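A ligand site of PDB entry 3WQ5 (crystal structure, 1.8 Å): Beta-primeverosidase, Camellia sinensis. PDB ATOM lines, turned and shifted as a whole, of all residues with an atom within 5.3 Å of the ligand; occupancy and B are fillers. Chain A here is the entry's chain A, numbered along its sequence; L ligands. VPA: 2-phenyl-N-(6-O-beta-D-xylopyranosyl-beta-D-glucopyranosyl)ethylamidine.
The side-chain amide oxygen (OE1) of Gln 53 lies within hydrogen-bond range of an oxygen (O3') of the ligand (2.6 Å).
The side-chain carboxylate (OE1) of Glu 203 is in salt-bridge range of a nitrogen (N1) of the ligand (2.6 Å).
The backbone carbonyl oxygen (O) of Glu 470 lies within hydrogen-bond range of an oxygen (O3A) of the ligand (2.9 Å).
O4' of the ligand lies within hydrogen-bond range of OE1 of Glu 470.
The side-chain carboxylate (OE2) of Glu 416 lies within hydrogen-bond range of an oxygen (O2') of the ligand, at 2.7 Å.
The side-chain amide oxygen (OE1) of Gln 477 is in hydrogen-bond range of an oxygen (O4A) of the ligand, at 2.7 Å.
OG of Ser 473 sits at hydrogen-bond distance from O3A of the ligand, 2.7 Å away.
NE1 of Trp 471 is in hydrogen-bond range of O3' of the ligand, at 2.9 Å.
The side-chain amide nitrogen (ND2) of Asn 202 is in hydrogen-bond range of an oxygen (O2') of the ligand (2.9 Å).
O4' of the ligand lies close to NE1 of Trp 463, at 3.1 Å.
An oxygen (O3') of the ligand is in hydrogen-bond range of a ring nitrogen (NE2) of His 157, 3.0 Å away.
OH of Tyr 345 sits close to O5' of the ligand (3.2 Å).
The indole nitrogen (NE1) of Trp 471 lies close to the side-chain amide nitrogen (NE2) of Gln 53 (3.1 Å).
The side-chain amide oxygen of Asn 468 lies within hydrogen-bond range of the side-chain amide nitrogen of Gln 53.
The side-chain amide oxygen of Gln 53 is in hydrogen-bond range of the side-chain hydroxyl of Ser 50, at 2.7 Å.
The side-chain carboxylate (OE2) of Glu 203 sits at hydrogen-bond distance from the side-chain amide nitrogen (ND2) of Asn 343 (2.8 Å).
NE1 of Trp 463 lies within hydrogen-bond range of OE2 of Glu 470 (3.1 Å).
The side-chain amide oxygen (OD1) of Asn 202 lies close to the side-chain carboxylate (OE2) of Glu 416 (3.2 Å).
The side-chain amide oxygen of Gln 477 is in hydrogen-bond range of the side-chain hydroxyl of Ser 473 (3.3 Å).
ND2 of Asn 202 is in hydrogen-bond range of NE2 of His 157 (3.1 Å).
Trp 158 touches the ligand (CH2 to C8, 3.9 Å).
Trp 205 touches the ligand.
Ser 206 touches the ligand.
Asn 343 touches the ligand.
Val 386 touches the ligand (CG1 to O4A, 3.97 Å).
Phe 389 touches the ligand.
Phe 479 touches the ligand (CZ to O5A, 3.7 Å).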
ATOM      1  N   SER A  50     -14.208  24.224 -21.141  1.00  0.00           N
ATOM      2  CA  SER A  50     -12.878  24.403 -21.729  1.00  0.00           C
ATOM      3  C   SER A  50     -12.733  25.843 -22.214  1.00  0.00           C
ATOM      4  O   SER A  50     -13.727  26.512 -22.491  1.00  0.00           O
ATOM      5  CB  SER A  50     -12.633  23.408 -22.880  1.00  0.00           C
ATOM      6  OG  SER A  50     -12.985  23.955 -24.138  1.00  0.00           O
ATOM      7  N   GLN A  53     -14.008  27.035 -25.757  1.00  0.00           N
ATOM      8  CA  GLN A  53     -15.440  26.830 -25.906  1.00  0.00           C
ATOM      9  C   GLN A  53     -16.283  27.791 -25.055  1.00  0.00           C
ATOM     10  O   GLN A  53     -17.462  28.002 -25.363  1.00  0.00           O
ATOM     11  CB  GLN A  53     -15.795  25.378 -25.541  1.00  0.00           C
ATOM     12  CG  GLN A  53     -15.079  24.365 -26.426  1.00  0.00           C
ATOM     13  CD  GLN A  53     -15.440  22.942 -26.066  1.00  0.00           C
ATOM     14  OE1 GLN A  53     -14.739  22.289 -25.314  1.00  0.00           O
ATOM     15  NE2 GLN A  53     -16.549  22.459 -26.616  1.00  0.00           N
ATOM     16  N   HIS A 157      -6.427  21.924 -23.710  1.00  0.00           N
ATOM     17  CA  HIS A 157      -7.692  21.457 -24.291  1.00  0.00           C
ATOM     18  C   HIS A 157      -7.808  21.968 -25.727  1.00  0.00           C
ATOM     19  O   HIS A 157      -8.784  22.625 -26.092  1.00  0.00           O
ATOM     20  CB  HIS A 157      -8.873  21.922 -23.424  1.00  0.00           C
ATOM     21  CG  HIS A 157     -10.138  21.135 -23.625  1.00  0.00           C
ATOM     22  ND1 HIS A 157     -10.825  20.554 -22.584  1.00  0.00           N
ATOM     23  CD2 HIS A 157     -10.854  20.865 -24.751  1.00  0.00           C
ATOM     24  CE1 HIS A 157     -11.905  19.952 -23.048  1.00  0.00           C
ATOM     25  NE2 HIS A 157     -11.945  20.125 -24.364  1.00  0.00           N
ATOM     26  N   TRP A 158      -6.752  21.695 -26.491  1.00  0.00           N
ATOM     27  CA  TRP A 158      -6.682  21.786 -27.962  1.00  0.00           C
ATOM     28  C   TRP A 158      -6.321  23.160 -28.521  1.00  0.00           C
ATOM     29  O   TRP A 158      -6.042  23.279 -29.714  1.00  0.00           O
ATOM     30  CB  TRP A 158      -7.992  21.340 -28.637  1.00  0.00           C
ATOM     31  CG  TRP A 158      -8.557  20.026 -28.214  1.00  0.00           C
ATOM     32  CD1 TRP A 158      -7.987  19.091 -27.379  1.00  0.00           C
ATOM     33  CD2 TRP A 158      -9.827  19.501 -28.588  1.00  0.00           C
ATOM     34  NE1 TRP A 158      -8.843  18.025 -27.222  1.00  0.00           N
ATOM     35  CE2 TRP A 158      -9.975  18.247 -27.950  1.00  0.00           C
ATOM     36  CE3 TRP A 158     -10.868  19.974 -29.397  1.00  0.00           C
ATOM     37  CZ2 TRP A 158     -11.125  17.469 -28.105  1.00  0.00           C
ATOM     38  CZ3 TRP A 158     -12.006  19.187 -29.553  1.00  0.00           C
ATOM     39  CH2 TRP A 158     -12.120  17.945 -28.910  1.00  0.00           C
ATOM     40  N   ASN A 202      -6.633  17.208 -22.678  1.00  0.00           N
ATOM     41  CA  ASN A 202      -7.934  16.626 -22.954  1.00  0.00           C
ATOM     42  C   ASN A 202      -7.929  15.864 -24.267  1.00  0.00           C
ATOM     43  O   ASN A 202      -7.654  16.440 -25.312  1.00  0.00           O
ATOM     44  CB  ASN A 202      -9.020  17.714 -23.005  1.00  0.00           C
ATOM     45  CG  ASN A 202     -10.396  17.139 -23.311  1.00  0.00           C
ATOM     46  OD1 ASN A 202     -11.055  16.569 -22.428  1.00  0.00           O
ATOM     47  ND2 ASN A 202     -10.829  17.274 -24.553  1.00  0.00           N
ATOM     48  N   GLU A 203      -8.231  14.574 -24.188  1.00  0.00           N
ATOM     49  CA  GLU A 203      -8.490  13.754 -25.371  1.00  0.00           C
ATOM     50  C   GLU A 203      -7.489  13.904 -26.501  1.00  0.00           C
ATOM     51  O   GLU A 203      -7.811  14.421 -27.566  1.00  0.00           O
ATOM     52  CB  GLU A 203      -9.885  14.071 -25.922  1.00  0.00           C
ATOM     53  CG  GLU A 203     -11.020  13.846 -24.931  1.00  0.00           C
ATOM     54  CD  GLU A 203     -12.373  14.098 -25.563  1.00  0.00           C
ATOM     55  OE1 GLU A 203     -12.415  14.628 -26.696  1.00  0.00           O
ATOM     56  OE2 GLU A 203     -13.397  13.770 -24.942  1.00  0.00           O
ATOM     57  N   TRP A 205      -6.714  11.674 -28.392  1.00  0.00           N
ATOM     58  CA  TRP A 205      -7.340  10.991 -29.530  1.00  0.00           C
ATOM     59  C   TRP A 205      -8.059  11.971 -30.440  1.00  0.00           C
ATOM     60  O   TRP A 205      -7.912  11.918 -31.661  1.00  0.00           O
ATOM     61  CB  TRP A 205      -8.339   9.907 -29.087  1.00  0.00           C
ATOM     62  CG  TRP A 205      -9.036   9.304 -30.287  1.00  0.00           C
ATOM     63  CD1 TRP A 205      -8.576   8.283 -31.065  1.00  0.00           C
ATOM     64  CD2 TRP A 205     -10.293   9.709 -30.854  1.00  0.00           C
ATOM     65  NE1 TRP A 205      -9.473   8.011 -32.070  1.00  0.00           N
ATOM     66  CE2 TRP A 205     -10.536   8.878 -31.969  1.00  0.00           C
ATOM     67  CE3 TRP A 205     -11.237  10.692 -30.524  1.00  0.00           C
ATOM     68  CZ2 TRP A 205     -11.680   9.003 -32.752  1.00  0.00           C
ATOM     69  CZ3 TRP A 205     -12.376  10.810 -31.295  1.00  0.00           C
ATOM     70  CH2 TRP A 205     -12.591   9.968 -32.401  1.00  0.00           C
ATOM     71  N   SER A 206      -8.864  12.847 -29.856  1.00  0.00           N
ATOM     72  CA  SER A 206      -9.627  13.798 -30.644  1.00  0.00           C
ATOM     73  C   SER A 206      -8.700  14.743 -31.377  1.00  0.00           C
ATOM     74  O   SER A 206      -8.926  15.062 -32.537  1.00  0.00           O
ATOM     75  CB  SER A 206     -10.602  14.592 -29.764  1.00  0.00           C
ATOM     76  OG  SER A 206     -11.513  13.740 -29.098  1.00  0.00           O
ATOM     77  N   TYR A 209      -6.921  12.451 -34.251  1.00  0.00           N
ATOM     78  CA  TYR A 209      -7.875  11.999 -35.255  1.00  0.00           C
ATOM     79  C   TYR A 209      -8.562  13.181 -35.933  1.00  0.00           C
ATOM     80  O   TYR A 209      -8.630  13.254 -37.165  1.00  0.00           O
ATOM     81  CB  TYR A 209      -8.929  11.063 -34.641  1.00  0.00           C
ATOM     82  CG  TYR A 209     -10.133  10.921 -35.547  1.00  0.00           C
ATOM     83  CD1 TYR A 209     -10.074  10.127 -36.685  1.00  0.00           C
ATOM     84  CD2 TYR A 209     -11.315  11.623 -35.284  1.00  0.00           C
ATOM     85  CE1 TYR A 209     -11.173  10.016 -37.527  1.00  0.00           C
ATOM     86  CE2 TYR A 209     -12.400  11.518 -36.127  1.00  0.00           C
ATOM     87  CZ  TYR A 209     -12.329  10.715 -37.248  1.00  0.00           C
ATOM     88  OH  TYR A 209     -13.425  10.617 -38.072  1.00  0.00           O
ATOM     89  N   LEU A 217     -11.073  19.099 -37.069  1.00  0.00           N
ATOM     90  CA  LEU A 217     -10.679  20.004 -35.995  1.00  0.00           C
ATOM     91  C   LEU A 217      -9.407  20.741 -36.387  1.00  0.00           C
ATOM     92  O   LEU A 217      -8.681  20.297 -37.278  1.00  0.00           O
ATOM     93  CB  LEU A 217     -10.439  19.216 -34.694  1.00  0.00           C
ATOM     94  CG  LEU A 217     -11.573  18.346 -34.148  1.00  0.00           C
ATOM     95  CD1 LEU A 217     -11.141  17.663 -32.872  1.00  0.00           C
ATOM     96  CD2 LEU A 217     -12.843  19.164 -33.933  1.00  0.00           C
ATOM     97  N   VAL A 273     -10.598   9.726 -24.079  1.00  0.00           N
ATOM     98  CA  VAL A 273     -11.963   9.438 -24.484  1.00  0.00           C
ATOM     99  C   VAL A 273     -11.969   8.155 -25.303  1.00  0.00           C
ATOM    100  O   VAL A 273     -11.010   7.861 -26.027  1.00  0.00           O
ATOM    101  CB  VAL A 273     -12.603  10.593 -25.299  1.00  0.00           C
ATOM    102  CG1 VAL A 273     -11.858  10.823 -26.614  1.00  0.00           C
ATOM    103  CG2 VAL A 273     -14.075  10.310 -25.570  1.00  0.00           C
ATOM    104  N   ASN A 343     -13.501  10.432 -20.349  1.00  0.00           N
ATOM    105  CA  ASN A 343     -14.687  11.052 -20.934  1.00  0.00           C
ATOM    106  C   ASN A 343     -15.561   9.975 -21.570  1.00  0.00           C
ATOM    107  O   ASN A 343     -15.098   9.241 -22.434  1.00  0.00           O
ATOM    108  CB  ASN A 343     -14.293  12.093 -21.990  1.00  0.00           C
ATOM    109  CG  ASN A 343     -13.643  13.333 -21.380  1.00  0.00           C
ATOM    110  OD1 ASN A 343     -13.531  13.448 -20.166  1.00  0.00           O
ATOM    111  ND2 ASN A 343     -13.198  14.248 -22.236  1.00  0.00           N
ATOM    112  N   TYR A 345     -19.299   9.170 -23.487  1.00  0.00           N
ATOM    113  CA  TYR A 345     -20.502   9.673 -24.123  1.00  0.00           C
ATOM    114  C   TYR A 345     -21.379   8.557 -24.668  1.00  0.00           C
ATOM    115  O   TYR A 345     -22.563   8.496 -24.350  1.00  0.00           O
ATOM    116  CB  TYR A 345     -20.159  10.650 -25.242  1.00  0.00           C
ATOM    117  CG  TYR A 345     -19.688  11.980 -24.710  1.00  0.00           C
ATOM    118  CD1 TYR A 345     -20.603  12.982 -24.421  1.00  0.00           C
ATOM    119  CD2 TYR A 345     -18.345  12.218 -24.468  1.00  0.00           C
ATOM    120  CE1 TYR A 345     -20.192  14.205 -23.907  1.00  0.00           C
ATOM    121  CE2 TYR A 345     -17.913  13.447 -23.967  1.00  0.00           C
ATOM    122  CZ  TYR A 345     -18.840  14.422 -23.684  1.00  0.00           C
ATOM    123  OH  TYR A 345     -18.418  15.637 -23.189  1.00  0.00           O
ATOM    124  N   VAL A 386     -27.881  15.037 -30.802  1.00  0.00           N
ATOM    125  CA  VAL A 386     -26.726  14.765 -31.630  1.00  0.00           C
ATOM    126  C   VAL A 386     -26.959  13.472 -32.407  1.00  0.00           C
ATOM    127  O   VAL A 386     -27.100  12.418 -31.801  1.00  0.00           O
ATOM    128  CB  VAL A 386     -25.430  14.637 -30.787  1.00  0.00           C
ATOM    129  CG1 VAL A 386     -24.231  14.413 -31.697  1.00  0.00           C
ATOM    130  CG2 VAL A 386     -25.243  15.867 -29.930  1.00  0.00           C
ATOM    131  N   PHE A 389     -25.082  10.276 -31.463  1.00  0.00           N
ATOM    132  CA  PHE A 389     -25.030   9.969 -30.038  1.00  0.00           C
ATOM    133  C   PHE A 389     -26.341   9.428 -29.490  1.00  0.00           C
ATOM    134  O   PHE A 389     -27.339  10.135 -29.447  1.00  0.00           O
ATOM    135  CB  PHE A 389     -24.631  11.210 -29.233  1.00  0.00           C
ATOM    136  CG  PHE A 389     -23.187  11.633 -29.389  1.00  0.00           C
ATOM    137  CD1 PHE A 389     -22.434  11.243 -30.487  1.00  0.00           C
ATOM    138  CD2 PHE A 389     -22.576  12.415 -28.420  1.00  0.00           C
ATOM    139  CE1 PHE A 389     -21.101  11.639 -30.620  1.00  0.00           C
ATOM    140  CE2 PHE A 389     -21.260  12.812 -28.546  1.00  0.00           C
ATOM    141  CZ  PHE A 389     -20.514  12.423 -29.649  1.00  0.00           C
ATOM    142  N   GLU A 416     -15.764  13.944 -18.129  1.00  0.00           N
ATOM    143  CA  GLU A 416     -16.891  14.403 -18.933  1.00  0.00           C
ATOM    144  C   GLU A 416     -17.936  13.311 -19.126  1.00  0.00           C
ATOM    145  O   GLU A 416     -17.609  12.177 -19.443  1.00  0.00           O
ATOM    146  CB  GLU A 416     -16.444  14.897 -20.328  1.00  0.00           C
ATOM    147  CG  GLU A 416     -15.654  16.198 -20.355  1.00  0.00           C
ATOM    148  CD  GLU A 416     -15.277  16.628 -21.743  1.00  0.00           C
ATOM    149  OE1 GLU A 416     -16.082  16.416 -22.676  1.00  0.00           O
ATOM    150  OE2 GLU A 416     -14.171  17.188 -21.919  1.00  0.00           O
ATOM    151  N   TRP A 463     -20.471  17.228 -18.568  1.00  0.00           N
ATOM    152  CA  TRP A 463     -20.307  18.102 -19.722  1.00  0.00           C
ATOM    153  C   TRP A 463     -21.692  18.447 -20.267  1.00  0.00           C
ATOM    154  O   TRP A 463     -22.384  17.562 -20.761  1.00  0.00           O
ATOM    155  CB  TRP A 463     -19.458  17.455 -20.831  1.00  0.00           C
ATOM    156  CG  TRP A 463     -19.219  18.461 -21.891  1.00  0.00           C
ATOM    157  CD1 TRP A 463     -20.020  18.730 -22.972  1.00  0.00           C
ATOM    158  CD2 TRP A 463     -18.164  19.425 -21.930  1.00  0.00           C
ATOM    159  NE1 TRP A 463     -19.506  19.776 -23.687  1.00  0.00           N
ATOM    160  CE2 TRP A 463     -18.368  20.218 -23.077  1.00  0.00           C
ATOM    161  CE3 TRP A 463     -17.054  19.678 -21.118  1.00  0.00           C
ATOM    162  CZ2 TRP A 463     -17.502  21.261 -23.426  1.00  0.00           C
ATOM    163  CZ3 TRP A 463     -16.186  20.700 -21.474  1.00  0.00           C
ATOM    164  CH2 TRP A 463     -16.416  21.481 -22.619  1.00  0.00           C
ATOM    165  N   ASN A 468     -22.324  25.920 -24.992  1.00  0.00           N
ATOM    166  CA  ASN A 468     -21.072  26.547 -25.411  1.00  0.00           C
ATOM    167  C   ASN A 468     -20.761  26.339 -26.886  1.00  0.00           C
ATOM    168  O   ASN A 468     -21.591  25.810 -27.629  1.00  0.00           O
ATOM    169  CB  ASN A 468     -19.924  25.999 -24.560  1.00  0.00           C
ATOM    170  CG  ASN A 468     -19.703  24.516 -24.770  1.00  0.00           C
ATOM    171  OD1 ASN A 468     -18.949  24.112 -25.660  1.00  0.00           O
ATOM    172  ND2 ASN A 468     -20.342  23.698 -23.944  1.00  0.00           N
ATOM    173  N   GLU A 470     -19.466  24.257 -29.455  1.00  0.00           N
ATOM    174  CA  GLU A 470     -19.167  22.834 -29.552  1.00  0.00           C
ATOM    175  C   GLU A 470     -18.364  22.510 -30.812  1.00  0.00           C
ATOM    176  O   GLU A 470     -18.814  21.759 -31.674  1.00  0.00           O
ATOM    177  CB  GLU A 470     -20.464  22.020 -29.514  1.00  0.00           C
ATOM    178  CG  GLU A 470     -21.173  22.083 -28.166  1.00  0.00           C
ATOM    179  CD  GLU A 470     -20.483  21.263 -27.085  1.00  0.00           C
ATOM    180  OE1 GLU A 470     -19.550  20.487 -27.417  1.00  0.00           O
ATOM    181  OE2 GLU A 470     -20.870  21.375 -25.905  1.00  0.00           O
ATOM    182  N   TRP A 471     -17.191  23.117 -30.897  1.00  0.00           N
ATOM    183  CA  TRP A 471     -16.211  22.833 -31.941  1.00  0.00           C
ATOM    184  C   TRP A 471     -16.839  22.871 -33.343  1.00  0.00           C
ATOM    185  O   TRP A 471     -17.427  23.883 -33.716  1.00  0.00           O
ATOM    186  CB  TRP A 471     -15.544  21.491 -31.662  1.00  0.00           C
ATOM    187  CG  TRP A 471     -14.895  21.423 -30.280  1.00  0.00           C
ATOM    188  CD1 TRP A 471     -15.221  20.569 -29.260  1.00  0.00           C
ATOM    189  CD2 TRP A 471     -13.833  22.253 -29.781  1.00  0.00           C
ATOM    190  NE1 TRP A 471     -14.428  20.805 -28.169  1.00  0.00           N
ATOM    191  CE2 TRP A 471     -13.566  21.845 -28.454  1.00  0.00           C
ATOM    192  CE3 TRP A 471     -13.088  23.307 -30.314  1.00  0.00           C
ATOM    193  CZ2 TRP A 471     -12.574  22.430 -27.678  1.00  0.00           C
ATOM    194  CZ3 TRP A 471     -12.107  23.899 -29.537  1.00  0.00           C
ATOM    195  CH2 TRP A 471     -11.862  23.452 -28.222  1.00  0.00           C
ATOM    196  N   LEU A 472     -16.738  21.782 -34.108  1.00  0.00           N
ATOM    197  CA  LEU A 472     -17.243  21.794 -35.483  1.00  0.00           C
ATOM    198  C   LEU A 472     -18.765  21.985 -35.586  1.00  0.00           C
ATOM    199  O   LEU A 472     -19.299  22.287 -36.653  1.00  0.00           O
ATOM    200  CB  LEU A 472     -16.825  20.512 -36.223  1.00  0.00           C
ATOM    201  CG  LEU A 472     -17.277  19.148 -35.704  1.00  0.00           C
ATOM    202  CD1 LEU A 472     -18.666  18.767 -36.222  1.00  0.00           C
ATOM    203  CD2 LEU A 472     -16.270  18.091 -36.094  1.00  0.00           C
ATOM    204  N   SER A 473     -19.473  21.809 -34.475  1.00  0.00           N
ATOM    205  CA  SER A 473     -20.931  21.956 -34.479  1.00  0.00           C
ATOM    206  C   SER A 473     -21.367  23.365 -34.068  1.00  0.00           C
ATOM    207  O   SER A 473     -22.564  23.658 -34.048  1.00  0.00           O
ATOM    208  CB  SER A 473     -21.578  20.928 -33.546  1.00  0.00           C
ATOM    209  OG  SER A 473     -21.333  19.608 -33.994  1.00  0.00           O
ATOM    210  N   GLN A 477     -25.534  22.725 -30.968  1.00  0.00           N
ATOM    211  CA  GLN A 477     -25.740  21.677 -29.987  1.00  0.00           C
ATOM    212  C   GLN A 477     -25.528  22.180 -28.578  1.00  0.00           C
ATOM    213  O   GLN A 477     -24.522  22.796 -28.276  1.00  0.00           O
ATOM    214  CB  GLN A 477     -24.857  20.472 -30.318  1.00  0.00           C
ATOM    215  CG  GLN A 477     -25.207  19.836 -31.644  1.00  0.00           C
ATOM    216  CD  GLN A 477     -24.234  18.763 -32.095  1.00  0.00           C
ATOM    217  OE1 GLN A 477     -23.218  18.527 -31.472  1.00  0.00           O
ATOM    218  NE2 GLN A 477     -24.557  18.101 -33.204  1.00  0.00           N
ATOM    219  N   PHE A 479     -25.085  21.259 -24.748  1.00  0.00           N
ATOM    220  CA  PHE A 479     -24.732  20.196 -23.795  1.00  0.00           C
ATOM    221  C   PHE A 479     -24.870  20.652 -22.343  1.00  0.00           C
ATOM    222  O   PHE A 479     -24.663  19.867 -21.428  1.00  0.00           O
ATOM    223  CB  PHE A 479     -23.293  19.734 -24.029  1.00  0.00           C
ATOM    224  CG  PHE A 479     -23.146  18.703 -25.124  1.00  0.00           C
ATOM    225  CD1 PHE A 479     -23.214  19.071 -26.453  1.00  0.00           C
ATOM    226  CD2 PHE A 479     -22.905  17.376 -24.801  1.00  0.00           C
ATOM    227  CE1 PHE A 479     -23.066  18.129 -27.457  1.00  0.00           C
ATOM    228  CE2 PHE A 479     -22.761  16.426 -25.800  1.00  0.00           C
ATOM    229  CZ  PHE A 479     -22.842  16.803 -27.128  1.00  0.00           C
HETATM  230  C1  VPA L   1     -15.458  14.996 -27.857  1.00  0.00           C
HETATM  231  C2  VPA L   1     -14.724  14.071 -28.833  1.00  0.00           C
HETATM  232  N2  VPA L   1     -16.575  15.621 -28.192  1.00  0.00           N
HETATM  233  C3  VPA L   1     -14.762  14.598 -30.296  1.00  0.00           C
HETATM  234  C4  VPA L   1     -14.568  13.688 -31.330  1.00  0.00           C
HETATM  235  C5  VPA L   1     -14.587  14.102 -32.654  1.00  0.00           C
HETATM  236  C6  VPA L   1     -14.801  15.440 -32.961  1.00  0.00           C
HETATM  237  C8  VPA L   1     -14.969  15.936 -30.614  1.00  0.00           C
HETATM  238  C7  VPA L   1     -14.991  16.356 -31.932  1.00  0.00           C
HETATM  239  N1  VPA L   1     -14.991  15.121 -26.624  1.00  0.00           N
HETATM  240  C1' VPA L   1     -15.633  16.016 -25.632  1.00  0.00           C
HETATM  241  O5' VPA L   1     -17.010  16.206 -26.045  1.00  0.00           O
HETATM  242  C2' VPA L   1     -14.726  17.260 -25.553  1.00  0.00           C
HETATM  243  O2' VPA L   1     -13.717  17.039 -24.569  1.00  0.00           O
HETATM  244  C3' VPA L   1     -15.505  18.541 -25.243  1.00  0.00           C
HETATM  245  O3' VPA L   1     -14.705  19.701 -25.519  1.00  0.00           O
HETATM  246  C4' VPA L   1     -16.745  18.565 -26.117  1.00  0.00           C
HETATM  247  O4' VPA L   1     -17.411  19.821 -25.994  1.00  0.00           O
HETATM  248  C5' VPA L   1     -17.659  17.431 -25.687  1.00  0.00           C
HETATM  249  C6' VPA L   1     -18.925  17.463 -26.519  1.00  0.00           C
HETATM  250  O6' VPA L   1     -18.444  17.235 -27.854  1.00  0.00           O
HETATM  251  C1A VPA L   1     -19.463  17.413 -28.827  1.00  0.00           C
HETATM  252  O5A VPA L   1     -19.938  16.115 -29.254  1.00  0.00           O
HETATM  253  C5A VPA L   1     -20.944  16.209 -30.284  1.00  0.00           C
HETATM  254  C4A VPA L   1     -20.345  16.896 -31.506  1.00  0.00           C
HETATM  255  O4A VPA L   1     -21.315  16.960 -32.562  1.00  0.00           O
HETATM  256  C3A VPA L   1     -19.908  18.306 -31.113  1.00  0.00           C
HETATM  257  O3A VPA L   1     -19.362  18.980 -32.234  1.00  0.00           O
HETATM  258  C2A VPA L   1     -18.866  18.192 -30.011  1.00  0.00           C
HETATM  259  O2A VPA L   1     -18.419  19.479 -29.601  1.00  0.00           O
